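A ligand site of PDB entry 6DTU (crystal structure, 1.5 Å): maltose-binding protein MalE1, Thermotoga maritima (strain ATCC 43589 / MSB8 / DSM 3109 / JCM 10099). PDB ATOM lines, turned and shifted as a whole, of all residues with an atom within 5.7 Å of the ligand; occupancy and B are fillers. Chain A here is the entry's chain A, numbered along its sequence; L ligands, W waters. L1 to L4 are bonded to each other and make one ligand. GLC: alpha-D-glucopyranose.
The side-chain carboxylate of Glu 109 sits at hydrogen-bond distance from the side-chain amide nitrogen of Gln 264 (2.9 Å). The backbone carbonyl oxygen (O) of Gly 262 lies within hydrogen-bond range of the backbone NH (N) of Glu 109, 2.9 Å away. OG of Ser 10 lies close to N of Lys 12 (3.2 Å). OE1 of Gln 13 is in hydrogen-bond range of OG of Ser 10 (2.7 Å). NE2 of Gln 13 sits close to NH2 of Arg 301, at 3.4 Å. The side-chain carboxylate (OD1) of Asp 299 lies within salt-bridge range of the guanidinium group (NE) of Arg 301. The backbone carbonyl oxygen (O) of Trp 231 lies close to the side-chain amino group (NZ) of Lys 12, 3.3 Å away. OH of Tyr 211 sits at hydrogen-bond distance from NE1 of Trp 231 (3.0 Å).
OE2 of Glu 109 sits at hydrogen-bond distance from O2 of GLC L2 (2.6 Å). The side-chain hydroxyl of Ser 10 is in hydrogen-bond range of an oxygen (O2) of GLC L1. The side-chain carboxylate of Asp 64 lies within hydrogen-bond range of an oxygen (O2) of GLC L3 (2.7 Å). O6 of GLC L2 sits at hydrogen-bond distance from OE2 of Glu 154 (2.8 Å). O of Gln 40 lies within hydrogen-bond range of O3 of GLC L4. The indole nitrogen (NE1) of Trp 65 sits at hydrogen-bond distance from an oxygen (O3) of GLC L3, 2.9 Å away. NH1 of Arg 301 sits at hydrogen-bond distance from O3 of GLC L1. O2 of GLC L2 lies within hydrogen-bond range of NE2 of Gln 264 (3.1 Å). OH of Tyr 157 is in hydrogen-bond range of O5 of GLC L2, 3.1 Å away.
CG of Lys 12 touches O2 of GLC L1 (3.5 Å). NE2 of Gln 13 touches O2 of GLC L1, at 3.9 Å. Phe 39 touches the ligand. CE of Lys 43 touches O2 of GLC L4 (3.6 Å). CB of Ala 62 touches O2 of GLC L3, at 3.4 Å. CD1 of Tyr 156 touches C1 of GLC L3, at 3.7 Å. CE2 of Tyr 211 touches O6 of GLC L1, 3.6 Å away. CZ2 of Trp 231 touches C1 of GLC L2, at 3.5 Å. Met 331 touches the ligand. Trp 341 touches the ligand. CB of Ala 342 touches O6 of GLC L4, at 3.8 Å. Within 4 Å of the ligand: Ser 10, Lys 12, Gln 13, Phe 39, Gln 40, Lys 43, Ala 62, Asp 64, Trp 65, Glu 109, Glu 154, Tyr 156, Tyr 157, Tyr 211, Trp 231, Gln 264, Arg 301, Met 331, Trp 341 and Ala 342. The nearest printed residue that does not touch the ligand is Ser 44 (4.04 Å).
Water W9 lies within hydrogen-bond range of O6 of GLC L4 (2.4 Å), O of Ala 338 (2.9 Å) and N of Ala 342 (3.0 Å). Water W2 lies within hydrogen-bond range of an oxygen (O4) of GLC L4 (2.7 Å), the backbone carbonyl oxygen (O) of Gln 40 (2.9 Å), the side-chain hydroxyl (OG) of Ser 44 (3.0 Å) and the side-chain carboxylate (OD1) of Asp 41 (3.5 Å). Water W8 lies within hydrogen-bond range of NZ of Lys 43 (2.8 Å), O3 of GLC L4 (2.8 Å) and N of Ser 44 (3.2 Å). Water W3 lies within hydrogen-bond range of the side-chain amide oxygen of Gln 40 (3.0 Å) and an oxygen (O6) of GLC L2 (3.0 Å). Water W7 lies within hydrogen-bond range of O of Phe 39 (2.8 Å), N of Lys 43 (2.9 Å), O2 of GLC L4 (3.0 Å), N of Ile 42 (3.4 Å) and O of Gln 40 (3.5 Å). Water W11 lies within hydrogen-bond range of the side-chain amide oxygen (OE1) of Gln 264, the side-chain amide nitrogen (NE2) of Gln 13 and an oxygen (O2) of GLC L1.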
ATOM      1  N   SER A  10     -15.758  -5.058 -10.338  1.00  0.00           N
ATOM      2  CA  SER A  10     -14.411  -5.148 -10.852  1.00  0.00           C
ATOM      3  C   SER A  10     -13.489  -5.773  -9.813  1.00  0.00           C
ATOM      4  O   SER A  10     -13.877  -6.051  -8.679  1.00  0.00           O
ATOM      5  CB  SER A  10     -13.890  -3.758 -11.218  1.00  0.00           C
ATOM      6  OG  SER A  10     -13.398  -3.102 -10.063  1.00  0.00           O
ATOM      7  N   GLU A  11     -12.219  -5.956 -10.187  1.00  0.00           N
ATOM      8  CA  GLU A  11     -11.275  -6.564  -9.255  1.00  0.00           C
ATOM      9  C   GLU A  11     -11.082  -5.738  -7.991  1.00  0.00           C
ATOM     10  O   GLU A  11     -10.750  -6.303  -6.941  1.00  0.00           O
ATOM     11  CB  GLU A  11      -9.917  -6.825  -9.916  1.00  0.00           C
ATOM     12  CG  GLU A  11      -9.113  -5.595 -10.223  1.00  0.00           C
ATOM     13  CD  GLU A  11      -9.284  -5.173 -11.645  1.00  0.00           C
ATOM     14  OE1 GLU A  11     -10.326  -5.545 -12.229  1.00  0.00           O
ATOM     15  OE2 GLU A  11      -8.378  -4.494 -12.199  1.00  0.00           O
ATOM     16  N   LYS A  12     -11.300  -4.424  -8.055  1.00  0.00           N
ATOM     17  CA  LYS A  12     -10.954  -3.557  -6.939  1.00  0.00           C
ATOM     18  C   LYS A  12     -11.824  -3.802  -5.717  1.00  0.00           C
ATOM     19  O   LYS A  12     -11.351  -3.636  -4.597  1.00  0.00           O
ATOM     20  CB  LYS A  12     -11.018  -2.090  -7.363  1.00  0.00           C
ATOM     21  CG  LYS A  12     -10.103  -1.716  -8.542  1.00  0.00           C
ATOM     22  CD  LYS A  12      -8.614  -1.992  -8.253  1.00  0.00           C
ATOM     23  CE  LYS A  12      -7.739  -1.601  -9.436  1.00  0.00           C
ATOM     24  NZ  LYS A  12      -6.288  -1.747  -9.101  1.00  0.00           N
ATOM     25  N   GLN A  13     -13.084  -4.175  -5.915  1.00  0.00           N
ATOM     26  CA  GLN A  13     -14.044  -4.294  -4.827  1.00  0.00           C
ATOM     27  C   GLN A  13     -14.248  -5.728  -4.355  1.00  0.00           C
ATOM     28  O   GLN A  13     -14.975  -5.931  -3.378  1.00  0.00           O
ATOM     29  CB  GLN A  13     -15.409  -3.675  -5.202  1.00  0.00           C
ATOM     30  CG  GLN A  13     -15.372  -2.240  -5.709  1.00  0.00           C
ATOM     31  CD  GLN A  13     -15.272  -2.143  -7.211  1.00  0.00           C
ATOM     32  OE1 GLN A  13     -15.029  -3.132  -7.901  1.00  0.00           O
ATOM     33  NE2 GLN A  13     -15.427  -0.943  -7.723  1.00  0.00           N
ATOM     34  N   PHE A  39     -14.134  -4.549 -15.664  1.00  0.00           N
ATOM     35  CA  PHE A  39     -14.992  -3.366 -15.536  1.00  0.00           C
ATOM     36  C   PHE A  39     -15.675  -3.013 -16.849  1.00  0.00           C
ATOM     37  O   PHE A  39     -16.891  -2.770 -16.879  1.00  0.00           O
ATOM     38  CB  PHE A  39     -14.209  -2.174 -14.993  1.00  0.00           C
ATOM     39  CG  PHE A  39     -15.045  -0.933 -14.930  1.00  0.00           C
ATOM     40  CD1 PHE A  39     -15.888  -0.707 -13.855  1.00  0.00           C
ATOM     41  CD2 PHE A  39     -15.065  -0.035 -15.987  1.00  0.00           C
ATOM     42  CE1 PHE A  39     -16.689   0.412 -13.784  1.00  0.00           C
ATOM     43  CE2 PHE A  39     -15.873   1.077 -15.930  1.00  0.00           C
ATOM     44  CZ  PHE A  39     -16.679   1.313 -14.835  1.00  0.00           C
ATOM     45  N   GLN A  40     -14.916  -2.933 -17.946  1.00  0.00           N
ATOM     46  CA  GLN A  40     -15.467  -2.577 -19.253  1.00  0.00           C
ATOM     47  C   GLN A  40     -16.426  -3.615 -19.781  1.00  0.00           C
ATOM     48  O   GLN A  40     -17.062  -3.364 -20.817  1.00  0.00           O
ATOM     49  CB  GLN A  40     -14.371  -2.473 -20.306  1.00  0.00           C
ATOM     50  CG  GLN A  40     -13.317  -1.394 -20.126  1.00  0.00           C
ATOM     51  CD  GLN A  40     -13.692  -0.038 -20.654  1.00  0.00           C
ATOM     52  OE1 GLN A  40     -13.868   0.909 -19.888  1.00  0.00           O
ATOM     53  NE2 GLN A  40     -13.777   0.091 -21.976  1.00  0.00           N
ATOM     54  N   ASP A  41     -16.537  -4.769 -19.144  1.00  0.00           N
ATOM     55  CA  ASP A  41     -17.456  -5.807 -19.569  1.00  0.00           C
ATOM     56  C   ASP A  41     -18.688  -5.915 -18.693  1.00  0.00           C
ATOM     57  O   ASP A  41     -19.628  -6.618 -19.057  1.00  0.00           O
ATOM     58  CB  ASP A  41     -16.727  -7.163 -19.632  1.00  0.00           C
ATOM     59  CG  ASP A  41     -15.735  -7.224 -20.770  1.00  0.00           C
ATOM     60  OD1 ASP A  41     -15.976  -6.552 -21.794  1.00  0.00           O
ATOM     61  OD2 ASP A  41     -14.703  -7.913 -20.640  1.00  0.00           O
ATOM     62  N   ILE A  42     -18.748  -5.197 -17.561  1.00  0.00           N
ATOM     63  CA  ILE A  42     -19.896  -5.359 -16.682  1.00  0.00           C
ATOM     64  C   ILE A  42     -21.194  -4.950 -17.360  1.00  0.00           C
ATOM     65  O   ILE A  42     -22.189  -5.682 -17.322  1.00  0.00           O
ATOM     66  CB  ILE A  42     -19.681  -4.572 -15.371  1.00  0.00           C
ATOM     67  CG1 ILE A  42     -18.560  -5.200 -14.543  1.00  0.00           C
ATOM     68  CG2 ILE A  42     -20.980  -4.485 -14.563  1.00  0.00           C
ATOM     69  CD1 ILE A  42     -18.213  -4.378 -13.280  1.00  0.00           C
ATOM     70  N   LYS A  43     -21.218  -3.749 -17.950  1.00  0.00           N
ATOM     71  CA  LYS A  43     -22.473  -3.260 -18.514  1.00  0.00           C
ATOM     72  C   LYS A  43     -22.903  -4.071 -19.728  1.00  0.00           C
ATOM     73  O   LYS A  43     -24.102  -4.363 -19.893  1.00  0.00           O
ATOM     74  CB  LYS A  43     -22.399  -1.773 -18.874  1.00  0.00           C
ATOM     75  CG  LYS A  43     -23.711  -1.307 -19.498  1.00  0.00           C
ATOM     76  CD  LYS A  43     -23.933   0.184 -19.349  1.00  0.00           C
ATOM     77  CE  LYS A  43     -22.951   0.989 -20.181  1.00  0.00           C
ATOM     78  NZ  LYS A  43     -23.142   0.821 -21.654  1.00  0.00           N
ATOM     79  N   SER A  44     -21.957  -4.398 -20.597  1.00  0.00           N
ATOM     80  CA  SER A  44     -22.290  -5.172 -21.792  1.00  0.00           C
ATOM     81  C   SER A  44     -22.759  -6.577 -21.430  1.00  0.00           C
ATOM     82  O   SER A  44     -23.748  -7.063 -21.991  1.00  0.00           O
ATOM     83  CB  SER A  44     -21.113  -5.182 -22.763  1.00  0.00           C
ATOM     84  OG  SER A  44     -19.923  -5.596 -22.109  1.00  0.00           O
ATOM     85  N   ALA A  62     -20.147   2.519 -12.721  1.00  0.00           N
ATOM     86  CA  ALA A  62     -20.125   3.974 -12.836  1.00  0.00           C
ATOM     87  C   ALA A  62     -21.480   4.559 -13.197  1.00  0.00           C
ATOM     88  O   ALA A  62     -22.325   3.895 -13.816  1.00  0.00           O
ATOM     89  CB  ALA A  62     -19.068   4.434 -13.837  1.00  0.00           C
ATOM     90  N   ASP A  64     -22.407   6.808 -15.293  1.00  0.00           N
ATOM     91  CA  ASP A  64     -22.790   7.047 -16.690  1.00  0.00           C
ATOM     92  C   ASP A  64     -23.679   5.937 -17.233  1.00  0.00           C
ATOM     93  O   ASP A  64     -24.376   6.150 -18.217  1.00  0.00           O
ATOM     94  CB  ASP A  64     -21.572   7.215 -17.607  1.00  0.00           C
ATOM     95  CG  ASP A  64     -20.688   5.964 -17.652  1.00  0.00           C
ATOM     96  OD1 ASP A  64     -20.083   5.653 -16.597  1.00  0.00           O
ATOM     97  OD2 ASP A  64     -20.594   5.329 -18.723  1.00  0.00           O
ATOM     98  N   TRP A  65     -23.676   4.765 -16.598  1.00  0.00           N
ATOM     99  CA  TRP A  65     -24.515   3.658 -17.045  1.00  0.00           C
ATOM    100  C   TRP A  65     -25.996   3.890 -16.754  1.00  0.00           C
ATOM    101  O   TRP A  65     -26.840   3.226 -17.373  1.00  0.00           O
ATOM    102  CB  TRP A  65     -24.147   2.378 -16.320  1.00  0.00           C
ATOM    103  CG  TRP A  65     -22.726   1.931 -16.385  1.00  0.00           C
ATOM    104  CD1 TRP A  65     -21.718   2.471 -17.133  1.00  0.00           C
ATOM    105  CD2 TRP A  65     -22.170   0.828 -15.670  1.00  0.00           C
ATOM    106  NE1 TRP A  65     -20.548   1.759 -16.928  1.00  0.00           N
ATOM    107  CE2 TRP A  65     -20.805   0.745 -16.032  1.00  0.00           C
ATOM    108  CE3 TRP A  65     -22.700  -0.101 -14.766  1.00  0.00           C
ATOM    109  CZ2 TRP A  65     -19.953  -0.248 -15.522  1.00  0.00           C
ATOM    110  CZ3 TRP A  65     -21.841  -1.087 -14.243  1.00  0.00           C
ATOM    111  CH2 TRP A  65     -20.479  -1.119 -14.602  1.00  0.00           C
ATOM    112  N   GLU A 109     -14.751  10.162  -8.090  1.00  0.00           N
ATOM    113  CA  GLU A 109     -13.384   9.962  -8.523  1.00  0.00           C
ATOM    114  C   GLU A 109     -13.113  10.844  -9.735  1.00  0.00           C
ATOM    115  O   GLU A 109     -14.038  11.286 -10.433  1.00  0.00           O
ATOM    116  CB  GLU A 109     -13.141   8.499  -8.913  1.00  0.00           C
ATOM    117  CG  GLU A 109     -14.016   8.081 -10.107  1.00  0.00           C
ATOM    118  CD  GLU A 109     -14.113   6.599 -10.299  1.00  0.00           C
ATOM    119  OE1 GLU A 109     -13.676   5.843  -9.403  1.00  0.00           O
ATOM    120  OE2 GLU A 109     -14.619   6.186 -11.352  1.00  0.00           O
ATOM    121  N   GLU A 154      -7.642   5.987 -25.488  1.00  0.00           N
ATOM    122  CA  GLU A 154      -8.870   5.767 -24.745  1.00  0.00           C
ATOM    123  C   GLU A 154      -9.436   7.124 -24.353  1.00  0.00           C
ATOM    124  O   GLU A 154      -8.827   7.857 -23.565  1.00  0.00           O
ATOM    125  CB  GLU A 154      -8.561   4.911 -23.522  1.00  0.00           C
ATOM    126  CG  GLU A 154      -9.742   4.171 -22.966  1.00  0.00           C
ATOM    127  CD  GLU A 154      -9.364   3.169 -21.883  1.00  0.00           C
ATOM    128  OE1 GLU A 154      -8.170   2.781 -21.769  1.00  0.00           O
ATOM    129  OE2 GLU A 154     -10.282   2.746 -21.150  1.00  0.00           O
ATOM    130  N   PHE A 155     -10.618   7.447 -24.882  1.00  0.00           N
ATOM    131  CA  PHE A 155     -11.196   8.782 -24.710  1.00  0.00           C
ATOM    132  C   PHE A 155     -11.282   9.202 -23.250  1.00  0.00           C
ATOM    133  O   PHE A 155     -11.036  10.378 -22.917  1.00  0.00           O
ATOM    134  CB  PHE A 155     -12.581   8.792 -25.361  1.00  0.00           C
ATOM    135  CG  PHE A 155     -13.424  10.011 -25.031  1.00  0.00           C
ATOM    136  CD1 PHE A 155     -12.943  11.286 -25.235  1.00  0.00           C
ATOM    137  CD2 PHE A 155     -14.732   9.855 -24.593  1.00  0.00           C
ATOM    138  CE1 PHE A 155     -13.708  12.389 -24.950  1.00  0.00           C
ATOM    139  CE2 PHE A 155     -15.518  10.966 -24.311  1.00  0.00           C
ATOM    140  CZ  PHE A 155     -15.011  12.238 -24.489  1.00  0.00           C
ATOM    141  N   TYR A 156     -11.664   8.282 -22.366  1.00  0.00           N
ATOM    142  CA  TYR A 156     -11.809   8.645 -20.954  1.00  0.00           C
ATOM    143  C   TYR A 156     -10.529   9.296 -20.396  1.00  0.00           C
ATOM    144  O   TYR A 156     -10.605  10.263 -19.625  1.00  0.00           O
ATOM    145  CB  TYR A 156     -12.227   7.412 -20.158  1.00  0.00           C
ATOM    146  CG  TYR A 156     -12.381   7.676 -18.678  1.00  0.00           C
ATOM    147  CD1 TYR A 156     -13.600   8.079 -18.120  1.00  0.00           C
ATOM    148  CD2 TYR A 156     -11.291   7.533 -17.817  1.00  0.00           C
ATOM    149  CE1 TYR A 156     -13.732   8.338 -16.743  1.00  0.00           C
ATOM    150  CE2 TYR A 156     -11.423   7.771 -16.434  1.00  0.00           C
ATOM    151  CZ  TYR A 156     -12.642   8.185 -15.926  1.00  0.00           C
ATOM    152  OH  TYR A 156     -12.752   8.417 -14.594  1.00  0.00           O
ATOM    153  N   TYR A 157      -9.365   8.805 -20.820  1.00  0.00           N
ATOM    154  CA  TYR A 157      -8.101   9.309 -20.303  1.00  0.00           C
ATOM    155  C   TYR A 157      -7.581  10.541 -21.047  1.00  0.00           C
ATOM    156  O   TYR A 157      -6.757  11.278 -20.487  1.00  0.00           O
ATOM    157  CB  TYR A 157      -7.046   8.181 -20.313  1.00  0.00           C
ATOM    158  CG  TYR A 157      -7.441   7.103 -19.335  1.00  0.00           C
ATOM    159  CD1 TYR A 157      -7.027   7.164 -18.012  1.00  0.00           C
ATOM    160  CD2 TYR A 157      -8.275   6.056 -19.724  1.00  0.00           C
ATOM    161  CE1 TYR A 157      -7.446   6.210 -17.091  1.00  0.00           C
ATOM    162  CE2 TYR A 157      -8.671   5.108 -18.818  1.00  0.00           C
ATOM    163  CZ  TYR A 157      -8.244   5.184 -17.510  1.00  0.00           C
ATOM    164  OH  TYR A 157      -8.642   4.256 -16.600  1.00  0.00           O
ATOM    165  N   TYR A 211      -4.311   0.938 -20.891  1.00  0.00           N
ATOM    166  CA  TYR A 211      -4.465   0.951 -19.445  1.00  0.00           C
ATOM    167  C   TYR A 211      -3.514  -0.048 -18.780  1.00  0.00           C
ATOM    168  O   TYR A 211      -2.856   0.282 -17.790  1.00  0.00           O
ATOM    169  CB  TYR A 211      -5.932   0.685 -19.047  1.00  0.00           C
ATOM    170  CG  TYR A 211      -6.075   0.852 -17.548  1.00  0.00           C
ATOM    171  CD1 TYR A 211      -6.285   2.112 -16.982  1.00  0.00           C
ATOM    172  CD2 TYR A 211      -5.898  -0.218 -16.703  1.00  0.00           C
ATOM    173  CE1 TYR A 211      -6.350   2.285 -15.603  1.00  0.00           C
ATOM    174  CE2 TYR A 211      -5.924  -0.043 -15.316  1.00  0.00           C
ATOM    175  CZ  TYR A 211      -6.145   1.216 -14.794  1.00  0.00           C
ATOM    176  OH  TYR A 211      -6.173   1.378 -13.442  1.00  0.00           O
ATOM    177  N   TRP A 231      -8.731   4.447  -8.017  1.00  0.00           N
ATOM    178  CA  TRP A 231      -8.865   2.993  -7.999  1.00  0.00           C
ATOM    179  C   TRP A 231      -7.526   2.289  -8.146  1.00  0.00           C
ATOM    180  O   TRP A 231      -7.447   1.090  -7.850  1.00  0.00           O
ATOM    181  CB  TRP A 231      -9.767   2.555  -9.161  1.00  0.00           C
ATOM    182  CG  TRP A 231      -9.322   3.076 -10.515  1.00  0.00           C
ATOM    183  CD1 TRP A 231      -8.360   2.540 -11.318  1.00  0.00           C
ATOM    184  CD2 TRP A 231      -9.816   4.241 -11.201  1.00  0.00           C
ATOM    185  NE1 TRP A 231      -8.228   3.290 -12.467  1.00  0.00           N
ATOM    186  CE2 TRP A 231      -9.105   4.342 -12.408  1.00  0.00           C
ATOM    187  CE3 TRP A 231     -10.774   5.216 -10.894  1.00  0.00           C
ATOM    188  CZ2 TRP A 231      -9.334   5.374 -13.336  1.00  0.00           C
ATOM    189  CZ3 TRP A 231     -11.015   6.223 -11.810  1.00  0.00           C
ATOM    190  CH2 TRP A 231     -10.274   6.316 -13.013  1.00  0.00           C
ATOM    191  N   GLY A 262     -16.505  10.916 -12.090  1.00  0.00           N
ATOM    192  CA  GLY A 262     -17.351   9.740 -12.073  1.00  0.00           C
ATOM    193  C   GLY A 262     -17.799   9.431 -10.655  1.00  0.00           C
ATOM    194  O   GLY A 262     -17.115   9.759  -9.692  1.00  0.00           O
ATOM    195  N   GLN A 264     -19.153   6.064  -8.411  1.00  0.00           N
ATOM    196  CA  GLN A 264     -19.248   4.602  -8.386  1.00  0.00           C
ATOM    197  C   GLN A 264     -20.303   4.221  -7.365  1.00  0.00           C
ATOM    198  O   GLN A 264     -20.422   4.859  -6.319  1.00  0.00           O
ATOM    199  CB  GLN A 264     -17.904   3.981  -7.964  1.00  0.00           C
ATOM    200  CG  GLN A 264     -16.742   4.225  -8.926  1.00  0.00           C
ATOM    201  CD  GLN A 264     -16.810   3.304 -10.125  1.00  0.00           C
ATOM    202  OE1 GLN A 264     -17.283   2.171 -10.041  1.00  0.00           O
ATOM    203  NE2 GLN A 264     -16.310   3.788 -11.256  1.00  0.00           N
ATOM    204  N   ASP A 299     -10.955   0.048  -1.007  1.00  0.00           N
ATOM    205  CA  ASP A 299     -10.989   0.565  -2.376  1.00  0.00           C
ATOM    206  C   ASP A 299     -11.018   2.087  -2.273  1.00  0.00           C
ATOM    207  O   ASP A 299     -12.071   2.708  -2.435  1.00  0.00           O
ATOM    208  CB  ASP A 299     -12.239   0.038  -3.096  1.00  0.00           C
ATOM    209  CG  ASP A 299     -12.422   0.576  -4.490  1.00  0.00           C
ATOM    210  OD1 ASP A 299     -11.483   1.184  -5.035  1.00  0.00           O
ATOM    211  OD2 ASP A 299     -13.526   0.371  -5.065  1.00  0.00           O
ATOM    212  N   ARG A 301     -11.230   5.736  -2.819  1.00  0.00           N
ATOM    213  CA  ARG A 301     -11.521   6.817  -3.758  1.00  0.00           C
ATOM    214  C   ARG A 301     -11.965   8.059  -2.961  1.00  0.00           C
ATOM    215  O   ARG A 301     -11.331   8.371  -1.949  1.00  0.00           O
ATOM    216  CB  ARG A 301     -12.533   6.345  -4.826  1.00  0.00           C
ATOM    217  CG  ARG A 301     -12.097   5.014  -5.427  1.00  0.00           C
ATOM    218  CD  ARG A 301     -12.995   4.492  -6.536  1.00  0.00           C
ATOM    219  NE  ARG A 301     -12.753   3.069  -6.790  1.00  0.00           N
ATOM    220  CZ  ARG A 301     -12.980   2.441  -7.947  1.00  0.00           C
ATOM    221  NH1 ARG A 301     -13.433   3.104  -9.027  1.00  0.00           N
ATOM    222  NH2 ARG A 301     -12.758   1.133  -7.996  1.00  0.00           N
ATOM    223  N   MET A 331     -19.358  12.995 -15.880  1.00  0.00           N
ATOM    224  CA  MET A 331     -19.813  12.241 -17.042  1.00  0.00           C
ATOM    225  C   MET A 331     -21.326  12.377 -17.140  1.00  0.00           C
ATOM    226  O   MET A 331     -22.010  12.375 -16.124  1.00  0.00           O
ATOM    227  CB  MET A 331     -19.476  10.749 -16.916  1.00  0.00           C
ATOM    228  CG  MET A 331     -18.035  10.390 -16.953  1.00  0.00           C
ATOM    229  SD  MET A 331     -17.786   8.603 -17.016  1.00  0.00           S
ATOM    230  CE  MET A 331     -18.159   8.105 -15.336  1.00  0.00           C
ATOM    231  N   ALA A 338     -23.960   6.105 -24.261  1.00  0.00           N
ATOM    232  CA  ALA A 338     -23.506   4.814 -24.764  1.00  0.00           C
ATOM    233  C   ALA A 338     -22.955   4.940 -26.187  1.00  0.00           C
ATOM    234  O   ALA A 338     -22.089   4.164 -26.588  1.00  0.00           O
ATOM    235  CB  ALA A 338     -24.652   3.798 -24.725  1.00  0.00           C
ATOM    236  N   TRP A 341     -18.467   6.497 -26.356  1.00  0.00           N
ATOM    237  CA  TRP A 341     -17.148   6.000 -25.991  1.00  0.00           C
ATOM    238  C   TRP A 341     -16.455   5.306 -27.164  1.00  0.00           C
ATOM    239  O   TRP A 341     -15.282   5.552 -27.428  1.00  0.00           O
ATOM    240  CB  TRP A 341     -17.279   5.022 -24.838  1.00  0.00           C
ATOM    241  CG  TRP A 341     -17.947   5.591 -23.607  1.00  0.00           C
ATOM    242  CD1 TRP A 341     -19.208   5.294 -23.164  1.00  0.00           C
ATOM    243  CD2 TRP A 341     -17.392   6.520 -22.664  1.00  0.00           C
ATOM    244  NE1 TRP A 341     -19.466   5.975 -22.010  1.00  0.00           N
ATOM    245  CE2 TRP A 341     -18.380   6.741 -21.673  1.00  0.00           C
ATOM    246  CE3 TRP A 341     -16.167   7.191 -22.564  1.00  0.00           C
ATOM    247  CZ2 TRP A 341     -18.180   7.578 -20.584  1.00  0.00           C
ATOM    248  CZ3 TRP A 341     -15.966   8.031 -21.485  1.00  0.00           C
ATOM    249  CH2 TRP A 341     -16.978   8.234 -20.514  1.00  0.00           C
ATOM    250  N   ALA A 342     -17.152   4.380 -27.831  1.00  0.00           N
ATOM    251  CA  ALA A 342     -16.514   3.587 -28.873  1.00  0.00           C
ATOM    252  C   ALA A 342     -16.093   4.449 -30.059  1.00  0.00           C
ATOM    253  O   ALA A 342     -15.014   4.240 -30.628  1.00  0.00           O
ATOM    254  CB  ALA A 342     -17.413   2.432 -29.314  1.00  0.00           C
ATOM    255  N   ASN A 345     -12.961   6.390 -28.860  1.00  0.00           N
ATOM    256  CA  ASN A 345     -11.824   5.475 -28.778  1.00  0.00           C
ATOM    257  C   ASN A 345     -11.290   5.166 -30.159  1.00  0.00           C
ATOM    258  O   ASN A 345     -10.073   5.147 -30.376  1.00  0.00           O
ATOM    259  CB  ASN A 345     -12.232   4.159 -28.106  1.00  0.00           C
ATOM    260  CG  ASN A 345     -12.442   4.292 -26.620  1.00  0.00           C
ATOM    261  OD1 ASN A 345     -12.088   5.295 -25.993  1.00  0.00           O
ATOM    262  ND2 ASN A 345     -13.000   3.268 -26.030  1.00  0.00           N
HETATM  263  C1  GLC L   1     -11.079  -0.884 -12.183  1.00  0.00           C
HETATM  264  C2  GLC L   1     -11.884   0.155 -11.512  1.00  0.00           C
HETATM  265  C3  GLC L   1     -12.668   0.941 -12.471  1.00  0.00           C
HETATM  266  C4  GLC L   1     -11.789   1.574 -13.496  1.00  0.00           C
HETATM  267  C5  GLC L   1     -11.026   0.477 -14.285  1.00  0.00           C
HETATM  268  C6  GLC L   1     -10.034   0.978 -15.141  1.00  0.00           C
HETATM  269  O1  GLC L   1     -11.916  -1.833 -12.769  1.00  0.00           O
HETATM  270  O2  GLC L   1     -12.764  -0.532 -10.565  1.00  0.00           O
HETATM  271  O3  GLC L   1     -13.375   1.974 -11.687  1.00  0.00           O
HETATM  272  O4  GLC L   1     -12.597   2.342 -14.433  1.00  0.00           O
HETATM  273  O5  GLC L   1     -10.246  -0.304 -13.220  1.00  0.00           O
HETATM  274  O6  GLC L   1      -9.501  -0.107 -15.911  1.00  0.00           O
HETATM  275  C1  GLC L   2     -12.162   3.660 -14.530  1.00  0.00           C
HETATM  276  C2  GLC L   2     -13.309   4.567 -14.280  1.00  0.00           C
HETATM  277  C3  GLC L   2     -14.404   4.301 -15.206  1.00  0.00           C
HETATM  278  C4  GLC L   2     -13.953   4.450 -16.644  1.00  0.00           C
HETATM  279  C5  GLC L   2     -12.719   3.547 -16.959  1.00  0.00           C
HETATM  280  C6  GLC L   2     -12.110   3.847 -18.220  1.00  0.00           C
HETATM  281  O2  GLC L   2     -13.803   4.281 -12.939  1.00  0.00           O
HETATM  282  O3  GLC L   2     -15.489   5.292 -15.027  1.00  0.00           O
HETATM  283  O4  GLC L   2     -15.022   3.996 -17.550  1.00  0.00           O
HETATM  284  O5  GLC L   2     -11.679   3.877 -15.891  1.00  0.00           O
HETATM  285  O6  GLC L   2     -11.224   2.798 -18.551  1.00  0.00           O
HETATM  286  C1  GLC L   3     -15.692   4.977 -18.278  1.00  0.00           C
HETATM  287  C2  GLC L   3     -17.140   4.696 -18.248  1.00  0.00           C
HETATM  288  C3  GLC L   3     -17.462   3.392 -18.904  1.00  0.00           C
HETATM  289  C4  GLC L   3     -17.026   3.359 -20.318  1.00  0.00           C
HETATM  290  C5  GLC L   3     -15.501   3.623 -20.420  1.00  0.00           C
HETATM  291  C6  GLC L   3     -15.082   3.755 -21.752  1.00  0.00           C
HETATM  292  O2  GLC L   3     -17.574   4.632 -16.859  1.00  0.00           O
HETATM  293  O3  GLC L   3     -18.910   3.153 -18.832  1.00  0.00           O
HETATM  294  O4  GLC L   3     -17.306   2.027 -20.835  1.00  0.00           O
HETATM  295  O5  GLC L   3     -15.200   4.966 -19.674  1.00  0.00           O
HETATM  296  O6  GLC L   3     -13.688   3.951 -21.752  1.00  0.00           O
HETATM  297  C1  GLC L   4     -18.401   1.977 -21.716  1.00  0.00           C
HETATM  298  C2  GLC L   4     -19.139   0.716 -21.467  1.00  0.00           C
HETATM  299  C3  GLC L   4     -18.345  -0.459 -21.912  1.00  0.00           C
HETATM  300  C4  GLC L   4     -17.951  -0.367 -23.355  1.00  0.00           C
HETATM  301  C5  GLC L   4     -17.080   0.877 -23.602  1.00  0.00           C
HETATM  302  C6  GLC L   4     -16.705   1.067 -24.982  1.00  0.00           C
HETATM  303  O2  GLC L   4     -19.414   0.610 -20.003  1.00  0.00           O
HETATM  304  O3  GLC L   4     -19.183  -1.641 -21.694  1.00  0.00           O
HETATM  305  O4  GLC L   4     -17.228  -1.550 -23.711  1.00  0.00           O
HETATM  306  O5  GLC L   4     -17.924   2.070 -23.120  1.00  0.00           O
HETATM  307  O6  GLC L   4     -17.874   1.201 -25.757  1.00  0.00           O
HETATM  308  O   HOH W   1     -12.522   1.934 -23.411  1.00  0.00           O
HETATM  309  O   HOH W   2     -17.752  -4.149 -23.562  1.00  0.00           O
HETATM  310  O   HOH W   3     -11.772  -0.064 -18.043  1.00  0.00           O
HETATM  311  O   HOH W   4     -12.913   5.953 -23.371  1.00  0.00           O
HETATM  312  O   HOH W   5      -8.449  -2.792 -15.450  1.00  0.00           O
HETATM  313  O   HOH W   6     -15.168   7.605 -13.574  1.00  0.00           O
HETATM  314  O   HOH W   7     -19.077  -1.876 -18.384  1.00  0.00           O
HETATM  315  O   HOH W   8     -21.956  -1.667 -22.272  1.00  0.00           O
HETATM  316  O   HOH W   9     -19.389   3.000 -26.426  1.00  0.00           O
HETATM  317  O   HOH W  10     -21.480   2.794 -22.498  1.00  0.00           O
HETATM  318  O   HOH W  11     -15.728   0.013 -10.498  1.00  0.00           O
